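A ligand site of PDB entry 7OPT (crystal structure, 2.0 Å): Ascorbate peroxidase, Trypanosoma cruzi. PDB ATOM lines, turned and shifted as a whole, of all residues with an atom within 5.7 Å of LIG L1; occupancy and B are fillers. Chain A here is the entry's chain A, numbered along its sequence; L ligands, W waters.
O2 of LG2 L2 is bound to FE1 of LIG L1 (2.3 Å).
The backbone NH (N) of Glu 221 is in hydrogen-bond range of an oxygen (O4) of LIG L1 (3.2 Å).
O2 of LIG L1 sits at hydrogen-bond distance from ND2 of Asn 226, 3.1 Å away.
O2 of LIG L1 is in salt-bridge range of NH1 of Arg 89 (3.7 Å).
An oxygen (O1) of LIG L1 is in hydrogen-bond range of the backbone NH (N) of His 223.
The side-chain hydroxyl (OG1) of Thr 227 lies within hydrogen-bond range of an oxygen (O1) of LIG L1, at 2.8 Å.
An oxygen (O1) of LG2 L2 lies within hydrogen-bond range of the guanidinium group of Arg 89.
An oxygen (O2) of LG2 L2 lies close to the indole nitrogen (NE1) of Trp 92.
NE2 of His 217 binds FE1 of LIG L1, at 2.4 Å.
O1 of LG2 L2 is in hydrogen-bond range of NE2 of His 93 (3.1 Å).
A ring nitrogen (ND1) of His 223 sits at hydrogen-bond distance from an oxygen (O2) of LIG L1 (2.8 Å).
The backbone carbonyl oxygen (O) of Tyr 229 sits at hydrogen-bond distance from the backbone NH (N) of Leu 224 (3.1 Å).
The backbone NH of Ala 277 sits at hydrogen-bond distance from the backbone carbonyl oxygen of Ala 189, at 2.7 Å.
A ring nitrogen (ND1) of His 223 is in hydrogen-bond range of the side-chain amide nitrogen (ND2) of Asn 226, 3.4 Å away.
The side-chain hydroxyl of Tyr 309 lies within hydrogen-bond range of the backbone carbonyl oxygen of Val 88, 3.0 Å away.
N of His 223 sits close to O of Tyr 229.
ND1 of His 217 sits at hydrogen-bond distance from NE1 of Trp 233, at 3.4 Å.
O of Ala 216 is in hydrogen-bond range of SG of Cys 219 (3.3 Å).
O of Lys 124 lies within hydrogen-bond range of NH2 of Arg 89, 3.0 Å away.
NE1 of Trp 92 lies close to N3 of LIG L1 (3.4 Å).
Pro 85 touches LIG L1 (O to C31, 3.1 Å).
CA of Leu 86 touches O3 of LIG L1, 3.6 Å away.
Val 88 touches LIG L1 (CB to C31, 3.9 Å).
Pro 187 touches LIG L1 (CB to C19, 3.5 Å).
Ala 189 touches LIG L1 (CA to C17, 3.5 Å).
Val 196 touches LIG L1.
Phe 200 touches LIG L1.
O of Leu 213 touches C24 of LIG L1 (3.6 Å).
Ile 214 touches LIG L1.
Ala 216 touches LIG L1 (CB to C25, 3.3 Å).
O of Cys 219 touches C31 of LIG L1 (3.97 Å).
Gly 220 touches LIG L1 (CA to O4, 3.1 Å).
Cys 222 touches LIG L1.
CD2 of Tyr 229 touches C9 of LIG L1, at 3.9 Å.
CH2 of Trp 233 touches C1 of LIG L1, at 3.3 Å.
CD1 of Leu 275 touches C2 of LIG L1, 3.7 Å away.
Ala 277 touches LIG L1 (CB to C17, 3.9 Å).
Tyr 309 touches LIG L1 (CE1 to C26, 3.7 Å).
Hydrophobic or aromatic side chains that line LIG L1: Pro 85, Leu 86, Val 88, Trp 92, Pro 187, Ala 189, Val 196, Phe 200, Leu 213, Ile 214, Ala 216, His 217, His 223, Tyr 229, Trp 233, Leu 275, Ala 277 and Tyr 309.
Within 4 Å of LIG L1: Pro 85, Leu 86, Val 88, Arg 89, Trp 92, Pro 187, Ala 189, Val 196, Phe 200, Leu 213, Ile 214, Ala 216, His 217, Cys 219, Gly 220, Glu 221, Cys 222, His 223, Asn 226, Thr 227, Tyr 229, Trp 233, Leu 275, Ala 277 and Tyr 309.
Along chain A the residues within 4 Å of LIG L1 span positions 85 to 309.
The nearest printed residue that does not touch LIG L1 is Asp 188 (4.1 Å).
Water W1 bridges a ring nitrogen (NE2) of His 93 and an oxygen (O1) of LG2 L2.
Water W2 bridges O1 of LG2 L2 (2.7 Å) and NE of Arg 89 (3.1 Å).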
ATOM      1  N   SER A  82     -17.182   4.884  -6.442  1.00  0.00           N
ATOM      2  CA  SER A  82     -17.451   4.295  -7.786  1.00  0.00           C
ATOM      3  C   SER A  82     -16.165   4.178  -8.611  1.00  0.00           C
ATOM      4  O   SER A  82     -16.220   3.534  -9.673  1.00  0.00           O
ATOM      5  CB  SER A  82     -18.450   5.064  -8.579  1.00  0.00           C
ATOM      6  OG  SER A  82     -17.859   6.234  -9.121  1.00  0.00           O
ATOM      7  N   PRO A  85     -13.853   0.241  -8.039  1.00  0.00           N
ATOM      8  CA  PRO A  85     -13.978  -0.916  -8.926  1.00  0.00           C
ATOM      9  C   PRO A  85     -13.424  -0.572 -10.299  1.00  0.00           C
ATOM     10  O   PRO A  85     -12.751  -1.429 -10.897  1.00  0.00           O
ATOM     11  CB  PRO A  85     -15.494  -1.212  -8.914  1.00  0.00           C
ATOM     12  CG  PRO A  85     -15.977  -0.574  -7.607  1.00  0.00           C
ATOM     13  CD  PRO A  85     -15.137   0.695  -7.495  1.00  0.00           C
ATOM     14  N   LEU A  86     -13.726   0.636 -10.749  1.00  0.00           N
ATOM     15  CA  LEU A  86     -13.318   1.195 -12.068  1.00  0.00           C
ATOM     16  C   LEU A  86     -11.802   1.130 -12.169  1.00  0.00           C
ATOM     17  O   LEU A  86     -11.240   0.709 -13.244  1.00  0.00           O
ATOM     18  CB  LEU A  86     -13.808   2.639 -12.157  1.00  0.00           C
ATOM     19  CG  LEU A  86     -13.072   3.486 -13.196  1.00  0.00           C
ATOM     20  CD1 LEU A  86     -13.478   3.058 -14.609  1.00  0.00           C
ATOM     21  CD2 LEU A  86     -13.319   4.972 -12.988  1.00  0.00           C
ATOM     22  N   VAL A  88      -9.948  -0.945 -10.534  1.00  0.00           N
ATOM     23  CA  VAL A  88      -9.600  -2.389 -10.656  1.00  0.00           C
ATOM     24  C   VAL A  88      -9.813  -2.860 -12.119  1.00  0.00           C
ATOM     25  O   VAL A  88      -9.001  -3.665 -12.595  1.00  0.00           O
ATOM     26  CB  VAL A  88     -10.409  -3.290  -9.708  1.00  0.00           C
ATOM     27  CG1 VAL A  88     -10.033  -4.739  -9.942  1.00  0.00           C
ATOM     28  CG2 VAL A  88     -10.257  -2.886  -8.243  1.00  0.00           C
ATOM     29  N   ARG A  89     -10.867  -2.414 -12.800  1.00  0.00           N
ATOM     30  CA  ARG A  89     -11.147  -2.743 -14.232  1.00  0.00           C
ATOM     31  C   ARG A  89     -10.021  -2.170 -15.125  1.00  0.00           C
ATOM     32  O   ARG A  89      -9.558  -2.897 -16.016  1.00  0.00           O
ATOM     33  CB  ARG A  89     -12.512  -2.199 -14.661  1.00  0.00           C
ATOM     34  CG  ARG A  89     -12.972  -2.594 -16.064  1.00  0.00           C
ATOM     35  CD  ARG A  89     -14.381  -2.132 -16.438  1.00  0.00           C
ATOM     36  NE  ARG A  89     -14.586  -2.257 -17.889  1.00  0.00           N
ATOM     37  CZ  ARG A  89     -14.976  -1.272 -18.703  1.00  0.00           C
ATOM     38  NH1 ARG A  89     -15.281  -0.087 -18.217  1.00  0.00           N
ATOM     39  NH2 ARG A  89     -15.084  -1.471 -20.009  1.00  0.00           N
ATOM     40  N   TRP A  92      -6.586  -4.075 -14.952  1.00  0.00           N
ATOM     41  CA  TRP A  92      -6.870  -5.429 -15.486  1.00  0.00           C
ATOM     42  C   TRP A  92      -6.905  -5.284 -16.994  1.00  0.00           C
ATOM     43  O   TRP A  92      -6.184  -6.061 -17.684  1.00  0.00           O
ATOM     44  CB  TRP A  92      -8.135  -6.036 -14.834  1.00  0.00           C
ATOM     45  CG  TRP A  92      -9.055  -6.854 -15.706  1.00  0.00           C
ATOM     46  CD1 TRP A  92     -10.412  -6.716 -15.748  1.00  0.00           C
ATOM     47  CD2 TRP A  92      -8.743  -7.969 -16.568  1.00  0.00           C
ATOM     48  NE1 TRP A  92     -10.954  -7.613 -16.629  1.00  0.00           N
ATOM     49  CE2 TRP A  92      -9.966  -8.402 -17.146  1.00  0.00           C
ATOM     50  CE3 TRP A  92      -7.562  -8.593 -17.018  1.00  0.00           C
ATOM     51  CZ2 TRP A  92     -10.045  -9.434 -18.092  1.00  0.00           C
ATOM     52  CZ3 TRP A  92      -7.645  -9.610 -17.938  1.00  0.00           C
ATOM     53  CH2 TRP A  92      -8.879 -10.036 -18.455  1.00  0.00           C
ATOM     54  N   HIS A  93      -7.619  -4.274 -17.472  1.00  0.00           N
ATOM     55  CA  HIS A  93      -7.744  -4.033 -18.923  1.00  0.00           C
ATOM     56  C   HIS A  93      -6.366  -3.654 -19.484  1.00  0.00           C
ATOM     57  O   HIS A  93      -6.058  -4.054 -20.650  1.00  0.00           O
ATOM     58  CB  HIS A  93      -8.942  -3.122 -19.219  1.00  0.00           C
ATOM     59  CG  HIS A  93     -10.160  -3.950 -19.450  1.00  0.00           C
ATOM     60  ND1 HIS A  93     -11.080  -3.651 -20.415  1.00  0.00           N
ATOM     61  CD2 HIS A  93     -10.570  -5.104 -18.862  1.00  0.00           C
ATOM     62  CE1 HIS A  93     -12.038  -4.571 -20.398  1.00  0.00           C
ATOM     63  NE2 HIS A  93     -11.748  -5.475 -19.456  1.00  0.00           N
ATOM     64  N   LYS A 124     -14.228   0.677 -23.240  1.00  0.00           N
ATOM     65  CA  LYS A 124     -15.112   1.876 -23.253  1.00  0.00           C
ATOM     66  C   LYS A 124     -15.507   2.194 -21.811  1.00  0.00           C
ATOM     67  O   LYS A 124     -15.736   1.242 -21.052  1.00  0.00           O
ATOM     68  CB  LYS A 124     -16.374   1.703 -24.121  1.00  0.00           C
ATOM     69  CG  LYS A 124     -17.112   3.015 -24.392  1.00  0.00           C
ATOM     70  CD  LYS A 124     -18.196   2.963 -25.472  1.00  0.00           C
ATOM     71  CE  LYS A 124     -19.047   4.228 -25.471  1.00  0.00           C
ATOM     72  NZ  LYS A 124     -20.173   4.173 -26.441  1.00  0.00           N
ATOM     73  N   PRO A 187     -11.814 -10.320 -23.095  1.00  0.00           N
ATOM     74  CA  PRO A 187     -12.925 -11.254 -23.219  1.00  0.00           C
ATOM     75  C   PRO A 187     -14.266 -10.612 -23.596  1.00  0.00           C
ATOM     76  O   PRO A 187     -14.549  -9.470 -23.275  1.00  0.00           O
ATOM     77  CB  PRO A 187     -13.035 -11.882 -21.845  1.00  0.00           C
ATOM     78  CG  PRO A 187     -12.376 -10.899 -20.883  1.00  0.00           C
ATOM     79  CD  PRO A 187     -11.368 -10.139 -21.701  1.00  0.00           C
ATOM     80  N   ASP A 188     -15.067 -11.405 -24.314  1.00  0.00           N
ATOM     81  CA  ASP A 188     -16.451 -11.146 -24.755  1.00  0.00           C
ATOM     82  C   ASP A 188     -17.362 -11.686 -23.646  1.00  0.00           C
ATOM     83  O   ASP A 188     -17.336 -12.883 -23.405  1.00  0.00           O
ATOM     84  CB  ASP A 188     -16.648 -11.810 -26.113  1.00  0.00           C
ATOM     85  CG  ASP A 188     -17.887 -11.401 -26.875  1.00  0.00           C
ATOM     86  OD1 ASP A 188     -18.810 -10.806 -26.263  1.00  0.00           O
ATOM     87  OD2 ASP A 188     -17.930 -11.704 -28.071  1.00  0.00           O
ATOM     88  N   ALA A 189     -18.130 -10.814 -22.995  1.00  0.00           N
ATOM     89  CA  ALA A 189     -19.057 -11.154 -21.894  1.00  0.00           C
ATOM     90  C   ALA A 189     -20.198 -12.017 -22.429  1.00  0.00           C
ATOM     91  O   ALA A 189     -20.598 -12.949 -21.699  1.00  0.00           O
ATOM     92  CB  ALA A 189     -19.612  -9.910 -21.271  1.00  0.00           C
ATOM     93  N   VAL A 196     -13.863 -17.829 -22.465  1.00  0.00           N
ATOM     94  CA  VAL A 196     -13.229 -17.496 -21.160  1.00  0.00           C
ATOM     95  C   VAL A 196     -11.904 -18.254 -21.023  1.00  0.00           C
ATOM     96  O   VAL A 196     -10.889 -17.616 -20.669  1.00  0.00           O
ATOM     97  CB  VAL A 196     -14.158 -17.823 -19.990  1.00  0.00           C
ATOM     98  CG1 VAL A 196     -13.413 -17.770 -18.673  1.00  0.00           C
ATOM     99  CG2 VAL A 196     -15.362 -16.911 -19.949  1.00  0.00           C
ATOM    100  N   PHE A 200      -8.020 -16.417 -20.846  1.00  0.00           N
ATOM    101  CA  PHE A 200      -7.179 -16.536 -19.620  1.00  0.00           C
ATOM    102  C   PHE A 200      -6.042 -17.557 -19.823  1.00  0.00           C
ATOM    103  O   PHE A 200      -5.047 -17.425 -19.083  1.00  0.00           O
ATOM    104  CB  PHE A 200      -8.041 -16.792 -18.377  1.00  0.00           C
ATOM    105  CG  PHE A 200      -8.840 -15.593 -17.958  1.00  0.00           C
ATOM    106  CD1 PHE A 200     -10.012 -15.249 -18.600  1.00  0.00           C
ATOM    107  CD2 PHE A 200      -8.378 -14.749 -16.954  1.00  0.00           C
ATOM    108  CE1 PHE A 200     -10.718 -14.117 -18.231  1.00  0.00           C
ATOM    109  CE2 PHE A 200      -9.084 -13.620 -16.571  1.00  0.00           C
ATOM    110  CZ  PHE A 200     -10.243 -13.284 -17.231  1.00  0.00           C
ATOM    111  N   LEU A 213      -9.872 -14.511 -10.442  1.00  0.00           N
ATOM    112  CA  LEU A 213      -9.821 -13.158 -11.049  1.00  0.00           C
ATOM    113  C   LEU A 213     -11.228 -12.704 -11.396  1.00  0.00           C
ATOM    114  O   LEU A 213     -11.548 -11.541 -11.105  1.00  0.00           O
ATOM    115  CB  LEU A 213      -8.901 -13.159 -12.271  1.00  0.00           C
ATOM    116  CG  LEU A 213      -7.415 -13.255 -11.941  1.00  0.00           C
ATOM    117  CD1 LEU A 213      -6.598 -13.641 -13.159  1.00  0.00           C
ATOM    118  CD2 LEU A 213      -6.888 -11.962 -11.318  1.00  0.00           C
ATOM    119  N   ILE A 214     -12.088 -13.610 -11.927  1.00  0.00           N
ATOM    120  CA  ILE A 214     -13.430 -13.162 -12.352  1.00  0.00           C
ATOM    121  C   ILE A 214     -14.234 -12.852 -11.081  1.00  0.00           C
ATOM    122  O   ILE A 214     -15.091 -11.978 -11.126  1.00  0.00           O
ATOM    123  CB  ILE A 214     -14.093 -14.140 -13.371  1.00  0.00           C
ATOM    124  CG1 ILE A 214     -13.200 -14.322 -14.608  1.00  0.00           C
ATOM    125  CG2 ILE A 214     -15.466 -13.647 -13.762  1.00  0.00           C
ATOM    126  CD1 ILE A 214     -13.679 -15.393 -15.558  1.00  0.00           C
ATOM    127  N   ALA A 216     -13.615 -10.753  -9.102  1.00  0.00           N
ATOM    128  CA  ALA A 216     -13.546  -9.281  -8.936  1.00  0.00           C
ATOM    129  C   ALA A 216     -14.912  -8.620  -9.168  1.00  0.00           C
ATOM    130  O   ALA A 216     -15.131  -7.486  -8.627  1.00  0.00           O
ATOM    131  CB  ALA A 216     -12.483  -8.692  -9.829  1.00  0.00           C
ATOM    132  N   HIS A 217     -15.832  -9.295  -9.865  1.00  0.00           N
ATOM    133  CA  HIS A 217     -17.212  -8.809 -10.140  1.00  0.00           C
ATOM    134  C   HIS A 217     -17.958  -8.651  -8.815  1.00  0.00           C
ATOM    135  O   HIS A 217     -18.986  -8.065  -8.806  1.00  0.00           O
ATOM    136  CB  HIS A 217     -17.931  -9.707 -11.129  1.00  0.00           C
ATOM    137  CG  HIS A 217     -17.459  -9.531 -12.511  1.00  0.00           C
ATOM    138  ND1 HIS A 217     -17.915 -10.263 -13.545  1.00  0.00           N
ATOM    139  CD2 HIS A 217     -16.574  -8.679 -13.030  1.00  0.00           C
ATOM    140  CE1 HIS A 217     -17.339  -9.878 -14.631  1.00  0.00           C
ATOM    141  NE2 HIS A 217     -16.563  -8.915 -14.344  1.00  0.00           N
ATOM    142  N   CYS A 219     -17.201  -6.582  -6.880  1.00  0.00           N
ATOM    143  CA  CYS A 219     -17.327  -5.106  -6.754  1.00  0.00           C
ATOM    144  C   CYS A 219     -17.582  -4.456  -8.104  1.00  0.00           C
ATOM    145  O   CYS A 219     -17.210  -5.038  -9.092  1.00  0.00           O
ATOM    146  CB  CYS A 219     -16.094  -4.445  -6.142  1.00  0.00           C
ATOM    147  SG  CYS A 219     -14.572  -4.606  -7.114  1.00  0.00           S
ATOM    148  N   GLY A 220     -18.100  -3.233  -8.079  1.00  0.00           N
ATOM    149  CA  GLY A 220     -18.521  -2.460  -9.244  1.00  0.00           C
ATOM    150  C   GLY A 220     -19.828  -2.977  -9.831  1.00  0.00           C
ATOM    151  O   GLY A 220     -20.525  -3.792  -9.188  1.00  0.00           O
ATOM    152  N   GLU A 221     -20.126  -2.485 -11.028  1.00  0.00           N
ATOM    153  CA  GLU A 221     -21.402  -2.705 -11.740  1.00  0.00           C
ATOM    154  C   GLU A 221     -21.169  -2.405 -13.209  1.00  0.00           C
ATOM    155  O   GLU A 221     -20.107  -1.795 -13.513  1.00  0.00           O
ATOM    156  CB  GLU A 221     -22.494  -1.803 -11.189  1.00  0.00           C
ATOM    157  CG  GLU A 221     -22.426  -0.355 -11.642  1.00  0.00           C
ATOM    158  CD  GLU A 221     -23.421   0.463 -10.825  1.00  0.00           C
ATOM    159  OE1 GLU A 221     -23.760   1.590 -11.228  1.00  0.00           O
ATOM    160  OE2 GLU A 221     -23.944  -0.097  -9.844  1.00  0.00           O
ATOM    161  N   CYS A 222     -22.099  -2.844 -14.066  1.00  0.00           N
ATOM    162  CA  CYS A 222     -22.051  -2.642 -15.543  1.00  0.00           C
ATOM    163  C   CYS A 222     -22.806  -1.338 -15.858  1.00  0.00           C
ATOM    164  O   CYS A 222     -23.700  -0.985 -15.111  1.00  0.00           O
ATOM    165  CB  CYS A 222     -22.651  -3.851 -16.272  1.00  0.00           C
ATOM    166  SG  CYS A 222     -21.749  -5.386 -15.986  1.00  0.00           S
ATOM    167  N   HIS A 223     -22.412  -0.617 -16.903  1.00  0.00           N
ATOM    168  CA  HIS A 223     -23.044   0.679 -17.270  1.00  0.00           C
ATOM    169  C   HIS A 223     -23.550   0.604 -18.700  1.00  0.00           C
ATOM    170  O   HIS A 223     -22.683   0.424 -19.592  1.00  0.00           O
ATOM    171  CB  HIS A 223     -22.021   1.821 -17.162  1.00  0.00           C
ATOM    172  CG  HIS A 223     -21.499   2.002 -15.794  1.00  0.00           C
ATOM    173  ND1 HIS A 223     -20.419   1.273 -15.316  1.00  0.00           N
ATOM    174  CD2 HIS A 223     -21.877   2.834 -14.809  1.00  0.00           C
ATOM    175  CE1 HIS A 223     -20.163   1.651 -14.075  1.00  0.00           C
ATOM    176  NE2 HIS A 223     -21.045   2.621 -13.745  1.00  0.00           N
ATOM    177  N   LEU A 224     -24.847   0.863 -18.912  1.00  0.00           N
ATOM    178  CA  LEU A 224     -25.520   0.838 -20.240  1.00  0.00           C
ATOM    179  C   LEU A 224     -24.591   1.545 -21.235  1.00  0.00           C
ATOM    180  O   LEU A 224     -24.271   0.958 -22.273  1.00  0.00           O
ATOM    181  CB  LEU A 224     -26.882   1.527 -20.123  1.00  0.00           C
ATOM    182  CG  LEU A 224     -27.822   1.425 -21.340  1.00  0.00           C
ATOM    183  CD1 LEU A 224     -28.101  -0.022 -21.708  1.00  0.00           C
ATOM    184  CD2 LEU A 224     -29.144   2.175 -21.107  1.00  0.00           C
ATOM    185  N   ASN A 226     -21.472   2.223 -21.220  1.00  0.00           N
ATOM    186  CA  ASN A 226     -20.144   1.590 -21.468  1.00  0.00           C
ATOM    187  C   ASN A 226     -20.282   0.312 -22.319  1.00  0.00           C
ATOM    188  O   ASN A 226     -19.582   0.242 -23.357  1.00  0.00           O
ATOM    189  CB  ASN A 226     -19.446   1.234 -20.155  1.00  0.00           C
ATOM    190  CG  ASN A 226     -19.005   2.455 -19.378  1.00  0.00           C
ATOM    191  OD1 ASN A 226     -18.894   3.559 -19.918  1.00  0.00           O
ATOM    192  ND2 ASN A 226     -18.719   2.253 -18.100  1.00  0.00           N
ATOM    193  N   THR A 227     -21.031  -0.693 -21.852  1.00  0.00           N
ATOM    194  CA  THR A 227     -21.051  -2.034 -22.483  1.00  0.00           C
ATOM    195  C   THR A 227     -22.498  -2.543 -22.718  1.00  0.00           C
ATOM    196  O   THR A 227     -22.653  -3.787 -22.815  1.00  0.00           O
ATOM    197  CB  THR A 227     -20.338  -3.054 -21.585  1.00  0.00           C
ATOM    198  OG1 THR A 227     -20.989  -2.898 -20.323  1.00  0.00           O
ATOM    199  CG2 THR A 227     -18.842  -2.840 -21.506  1.00  0.00           C
ATOM    200  N   GLY A 228     -23.501  -1.657 -22.636  1.00  0.00           N
ATOM    201  CA  GLY A 228     -24.934  -2.009 -22.803  1.00  0.00           C
ATOM    202  C   GLY A 228     -25.379  -3.104 -21.856  1.00  0.00           C
ATOM    203  O   GLY A 228     -26.442  -3.717 -22.085  1.00  0.00           O
ATOM    204  N   TYR A 229     -24.582  -3.376 -20.834  1.00  0.00           N
ATOM    205  CA  TYR A 229     -24.924  -4.256 -19.700  1.00  0.00           C
ATOM    206  C   TYR A 229     -25.146  -3.301 -18.510  1.00  0.00           C
ATOM    207  O   TYR A 229     -24.578  -2.167 -18.519  1.00  0.00           O
ATOM    208  CB  TYR A 229     -23.815  -5.293 -19.453  1.00  0.00           C
ATOM    209  CG  TYR A 229     -23.539  -6.312 -20.524  1.00  0.00           C
ATOM    210  CD1 TYR A 229     -24.460  -7.311 -20.827  1.00  0.00           C
ATOM    211  CD2 TYR A 229     -22.293  -6.383 -21.145  1.00  0.00           C
ATOM    212  CE1 TYR A 229     -24.158  -8.307 -21.747  1.00  0.00           C
ATOM    213  CE2 TYR A 229     -21.984  -7.355 -22.082  1.00  0.00           C
ATOM    214  CZ  TYR A 229     -22.911  -8.355 -22.378  1.00  0.00           C
ATOM    215  OH  TYR A 229     -22.615  -9.386 -23.241  1.00  0.00           O
ATOM    216  N   TRP A 233     -23.368  -6.886  -9.505  1.00  0.00           N
ATOM    217  CA  TRP A 233     -23.334  -8.349  -9.317  1.00  0.00           C
ATOM    218  C   TRP A 233     -23.773  -8.714  -7.897  1.00  0.00           C
ATOM    219  O   TRP A 233     -24.335  -9.789  -7.749  1.00  0.00           O
ATOM    220  CB  TRP A 233     -21.930  -8.893  -9.575  1.00  0.00           C
ATOM    221  CG  TRP A 233     -21.507  -8.784 -11.000  1.00  0.00           C
ATOM    222  CD1 TRP A 233     -21.709  -9.708 -11.971  1.00  0.00           C
ATOM    223  CD2 TRP A 233     -20.841  -7.680 -11.635  1.00  0.00           C
ATOM    224  NE1 TRP A 233     -21.192  -9.262 -13.156  1.00  0.00           N
ATOM    225  CE2 TRP A 233     -20.663  -8.023 -12.992  1.00  0.00           C
ATOM    226  CE3 TRP A 233     -20.364  -6.443 -11.191  1.00  0.00           C
ATOM    227  CZ2 TRP A 233     -20.025  -7.189 -13.904  1.00  0.00           C
ATOM    228  CZ3 TRP A 233     -19.713  -5.636 -12.082  1.00  0.00           C
ATOM    229  CH2 TRP A 233     -19.534  -5.995 -13.414  1.00  0.00           C
ATOM    230  N   LEU A 275     -23.518 -11.913 -16.337  1.00  0.00           N
ATOM    231  CA  LEU A 275     -23.182 -11.917 -17.779  1.00  0.00           C
ATOM    232  C   LEU A 275     -23.190 -13.350 -18.251  1.00  0.00           C
ATOM    233  O   LEU A 275     -22.910 -14.245 -17.467  1.00  0.00           O
ATOM    234  CB  LEU A 275     -21.780 -11.345 -17.956  1.00  0.00           C
ATOM    235  CG  LEU A 275     -21.593  -9.935 -17.447  1.00  0.00           C
ATOM    236  CD1 LEU A 275     -20.082  -9.631 -17.325  1.00  0.00           C
ATOM    237  CD2 LEU A 275     -22.293  -8.939 -18.338  1.00  0.00           C
ATOM    238  N   ALA A 277     -20.887 -14.818 -19.706  1.00  0.00           N
ATOM    239  CA  ALA A 277     -19.547 -15.299 -19.274  1.00  0.00           C
ATOM    240  C   ALA A 277     -19.552 -15.722 -17.796  1.00  0.00           C
ATOM    241  O   ALA A 277     -18.951 -16.775 -17.484  1.00  0.00           O
ATOM    242  CB  ALA A 277     -18.513 -14.225 -19.483  1.00  0.00           C
ATOM    243  N   PHE A 305      -7.040 -14.532  -5.157  1.00  0.00           N
ATOM    244  CA  PHE A 305      -7.193 -13.295  -5.943  1.00  0.00           C
ATOM    245  C   PHE A 305      -5.893 -12.496  -5.833  1.00  0.00           C
ATOM    246  O   PHE A 305      -5.322 -12.145  -6.862  1.00  0.00           O
ATOM    247  CB  PHE A 305      -8.386 -12.502  -5.422  1.00  0.00           C
ATOM    248  CG  PHE A 305      -8.520 -11.221  -6.183  1.00  0.00           C
ATOM    249  CD1 PHE A 305      -7.840 -10.090  -5.791  1.00  0.00           C
ATOM    250  CD2 PHE A 305      -9.211 -11.212  -7.386  1.00  0.00           C
ATOM    251  CE1 PHE A 305      -7.897  -8.937  -6.559  1.00  0.00           C
ATOM    252  CE2 PHE A 305      -9.321 -10.043  -8.118  1.00  0.00           C
ATOM    253  CZ  PHE A 305      -8.635  -8.925  -7.721  1.00  0.00           C
ATOM    254  N   TYR A 309      -3.965 -11.573  -9.088  1.00  0.00           N
ATOM    255  CA  TYR A 309      -4.092 -10.173  -9.535  1.00  0.00           C
ATOM    256  C   TYR A 309      -2.699  -9.551  -9.576  1.00  0.00           C
ATOM    257  O   TYR A 309      -2.393  -8.780 -10.502  1.00  0.00           O
ATOM    258  CB  TYR A 309      -5.027  -9.414  -8.620  1.00  0.00           C
ATOM    259  CG  TYR A 309      -5.469  -8.113  -9.236  1.00  0.00           C
ATOM    260  CD1 TYR A 309      -6.261  -8.091 -10.379  1.00  0.00           C
ATOM    261  CD2 TYR A 309      -5.052  -6.904  -8.701  1.00  0.00           C
ATOM    262  CE1 TYR A 309      -6.652  -6.894 -10.966  1.00  0.00           C
ATOM    263  CE2 TYR A 309      -5.448  -5.699  -9.278  1.00  0.00           C
ATOM    264  CZ  TYR A 309      -6.268  -5.691 -10.394  1.00  0.00           C
ATOM    265  OH  TYR A 309      -6.648  -4.497 -10.931  1.00  0.00           O
ATOM    266  N   LEU A 312      -1.125 -10.550 -12.583  1.00  0.00           N
ATOM    267  CA  LEU A 312      -1.765  -9.884 -13.749  1.00  0.00           C
ATOM    268  C   LEU A 312      -1.068  -8.541 -13.932  1.00  0.00           C
ATOM    269  O   LEU A 312      -0.724  -8.173 -15.084  1.00  0.00           O
ATOM    270  CB  LEU A 312      -3.272  -9.735 -13.488  1.00  0.00           C
ATOM    271  CG  LEU A 312      -4.114  -9.150 -14.635  1.00  0.00           C
ATOM    272  CD1 LEU A 312      -4.210 -10.106 -15.802  1.00  0.00           C
ATOM    273  CD2 LEU A 312      -5.522  -8.782 -14.164  1.00  0.00           C
HETATM  274  C1  LIG L   1     -16.950  -4.784 -14.981  1.00  0.00           C
HETATM  275  C2  LIG L   1     -16.797  -8.234 -18.358  1.00  0.00           C
HETATM  276  C3  LIG L   1     -13.212 -10.468 -15.961  1.00  0.00           C
HETATM  277  C4  LIG L   1     -13.233  -6.680 -12.952  1.00  0.00           C
HETATM  278  C5  LIG L   1     -17.184  -5.501 -16.111  1.00  0.00           C
HETATM  279  C6  LIG L   1     -18.049  -5.070 -17.126  1.00  0.00           C
HETATM  280  C7  LIG L   1     -18.026  -6.057 -18.081  1.00  0.00           C
HETATM  281  C8  LIG L   1     -17.148  -7.093 -17.676  1.00  0.00           C
HETATM  282  C9  LIG L   1     -18.855  -6.060 -19.316  1.00  0.00           C
HETATM  283  C10 LIG L   1     -18.915  -3.850 -17.106  1.00  0.00           C
HETATM  284  C11 LIG L   1     -18.211  -2.668 -17.775  1.00  0.00           C
HETATM  285  C12 LIG L   1     -19.012  -1.423 -17.541  1.00  0.00           C
HETATM  286  O1  LIG L   1     -20.075  -1.363 -18.201  1.00  0.00           O
HETATM  287  O2  LIG L   1     -18.670  -0.473 -16.724  1.00  0.00           O
HETATM  288  C13 LIG L   1     -15.799  -9.177 -17.951  1.00  0.00           C
HETATM  289  C14 LIG L   1     -15.544 -10.425 -18.588  1.00  0.00           C
HETATM  290  C15 LIG L   1     -14.608 -11.061 -17.897  1.00  0.00           C
HETATM  291  C16 LIG L   1     -14.251 -10.156 -16.815  1.00  0.00           C
HETATM  292  C17 LIG L   1     -16.244 -11.017 -19.779  1.00  0.00           C
HETATM  293  C18 LIG L   1     -13.942 -12.345 -18.098  1.00  0.00           C
HETATM  294  C19 LIG L   1     -14.369 -13.286 -18.923  1.00  0.00           C
HETATM  295  C20 LIG L   1     -12.799  -9.575 -14.979  1.00  0.00           C
HETATM  296  C21 LIG L   1     -11.621  -9.550 -14.282  1.00  0.00           C
HETATM  297  C22 LIG L   1     -11.671  -8.434 -13.425  1.00  0.00           C
HETATM  298  C23 LIG L   1     -12.874  -7.788 -13.648  1.00  0.00           C
HETATM  299  C24 LIG L   1     -10.451 -10.501 -14.360  1.00  0.00           C
HETATM  300  C25 LIG L   1     -10.640  -7.981 -12.447  1.00  0.00           C
HETATM  301  C26 LIG L   1      -9.537  -8.738 -12.239  1.00  0.00           C
HETATM  302  C27 LIG L   1     -14.277  -5.905 -13.253  1.00  0.00           C
HETATM  303  C28 LIG L   1     -14.633  -4.780 -12.415  1.00  0.00           C
HETATM  304  C29 LIG L   1     -15.676  -4.228 -13.026  1.00  0.00           C
HETATM  305  C30 LIG L   1     -15.940  -5.074 -14.164  1.00  0.00           C
HETATM  306  C31 LIG L   1     -13.921  -4.274 -11.173  1.00  0.00           C
HETATM  307  C32 LIG L   1     -16.478  -3.000 -12.592  1.00  0.00           C
HETATM  308  C33 LIG L   1     -16.211  -1.687 -13.322  1.00  0.00           C
HETATM  309  C34 LIG L   1     -16.870  -0.519 -12.604  1.00  0.00           C
HETATM  310  O3  LIG L   1     -16.787   0.684 -13.031  1.00  0.00           O
HETATM  311  O4  LIG L   1     -17.574  -0.712 -11.587  1.00  0.00           O
HETATM  312  N1  LIG L   1     -16.580  -6.689 -16.474  1.00  0.00           N
HETATM  313  N2  LIG L   1     -14.930  -9.055 -16.958  1.00  0.00           N
HETATM  314  N3  LIG L   1     -13.566  -8.484 -14.632  1.00  0.00           N
HETATM  315  N4  LIG L   1     -15.089  -6.096 -14.273  1.00  0.00           N
HETATM  316 FE1  LIG L   1     -15.029  -7.476 -15.575  1.00  0.00          FE
HETATM  317  O1  LG2 L   2     -14.115  -5.188 -17.541  1.00  0.00           O
HETATM  318  O2  LG2 L   2     -13.657  -6.097 -16.842  1.00  0.00           O
HETATM  319  O   HOH W   1     -13.317  -7.571 -19.284  1.00  0.00           O
HETATM  320  O   HOH W   2     -15.536  -4.548 -19.738  1.00  0.00           O
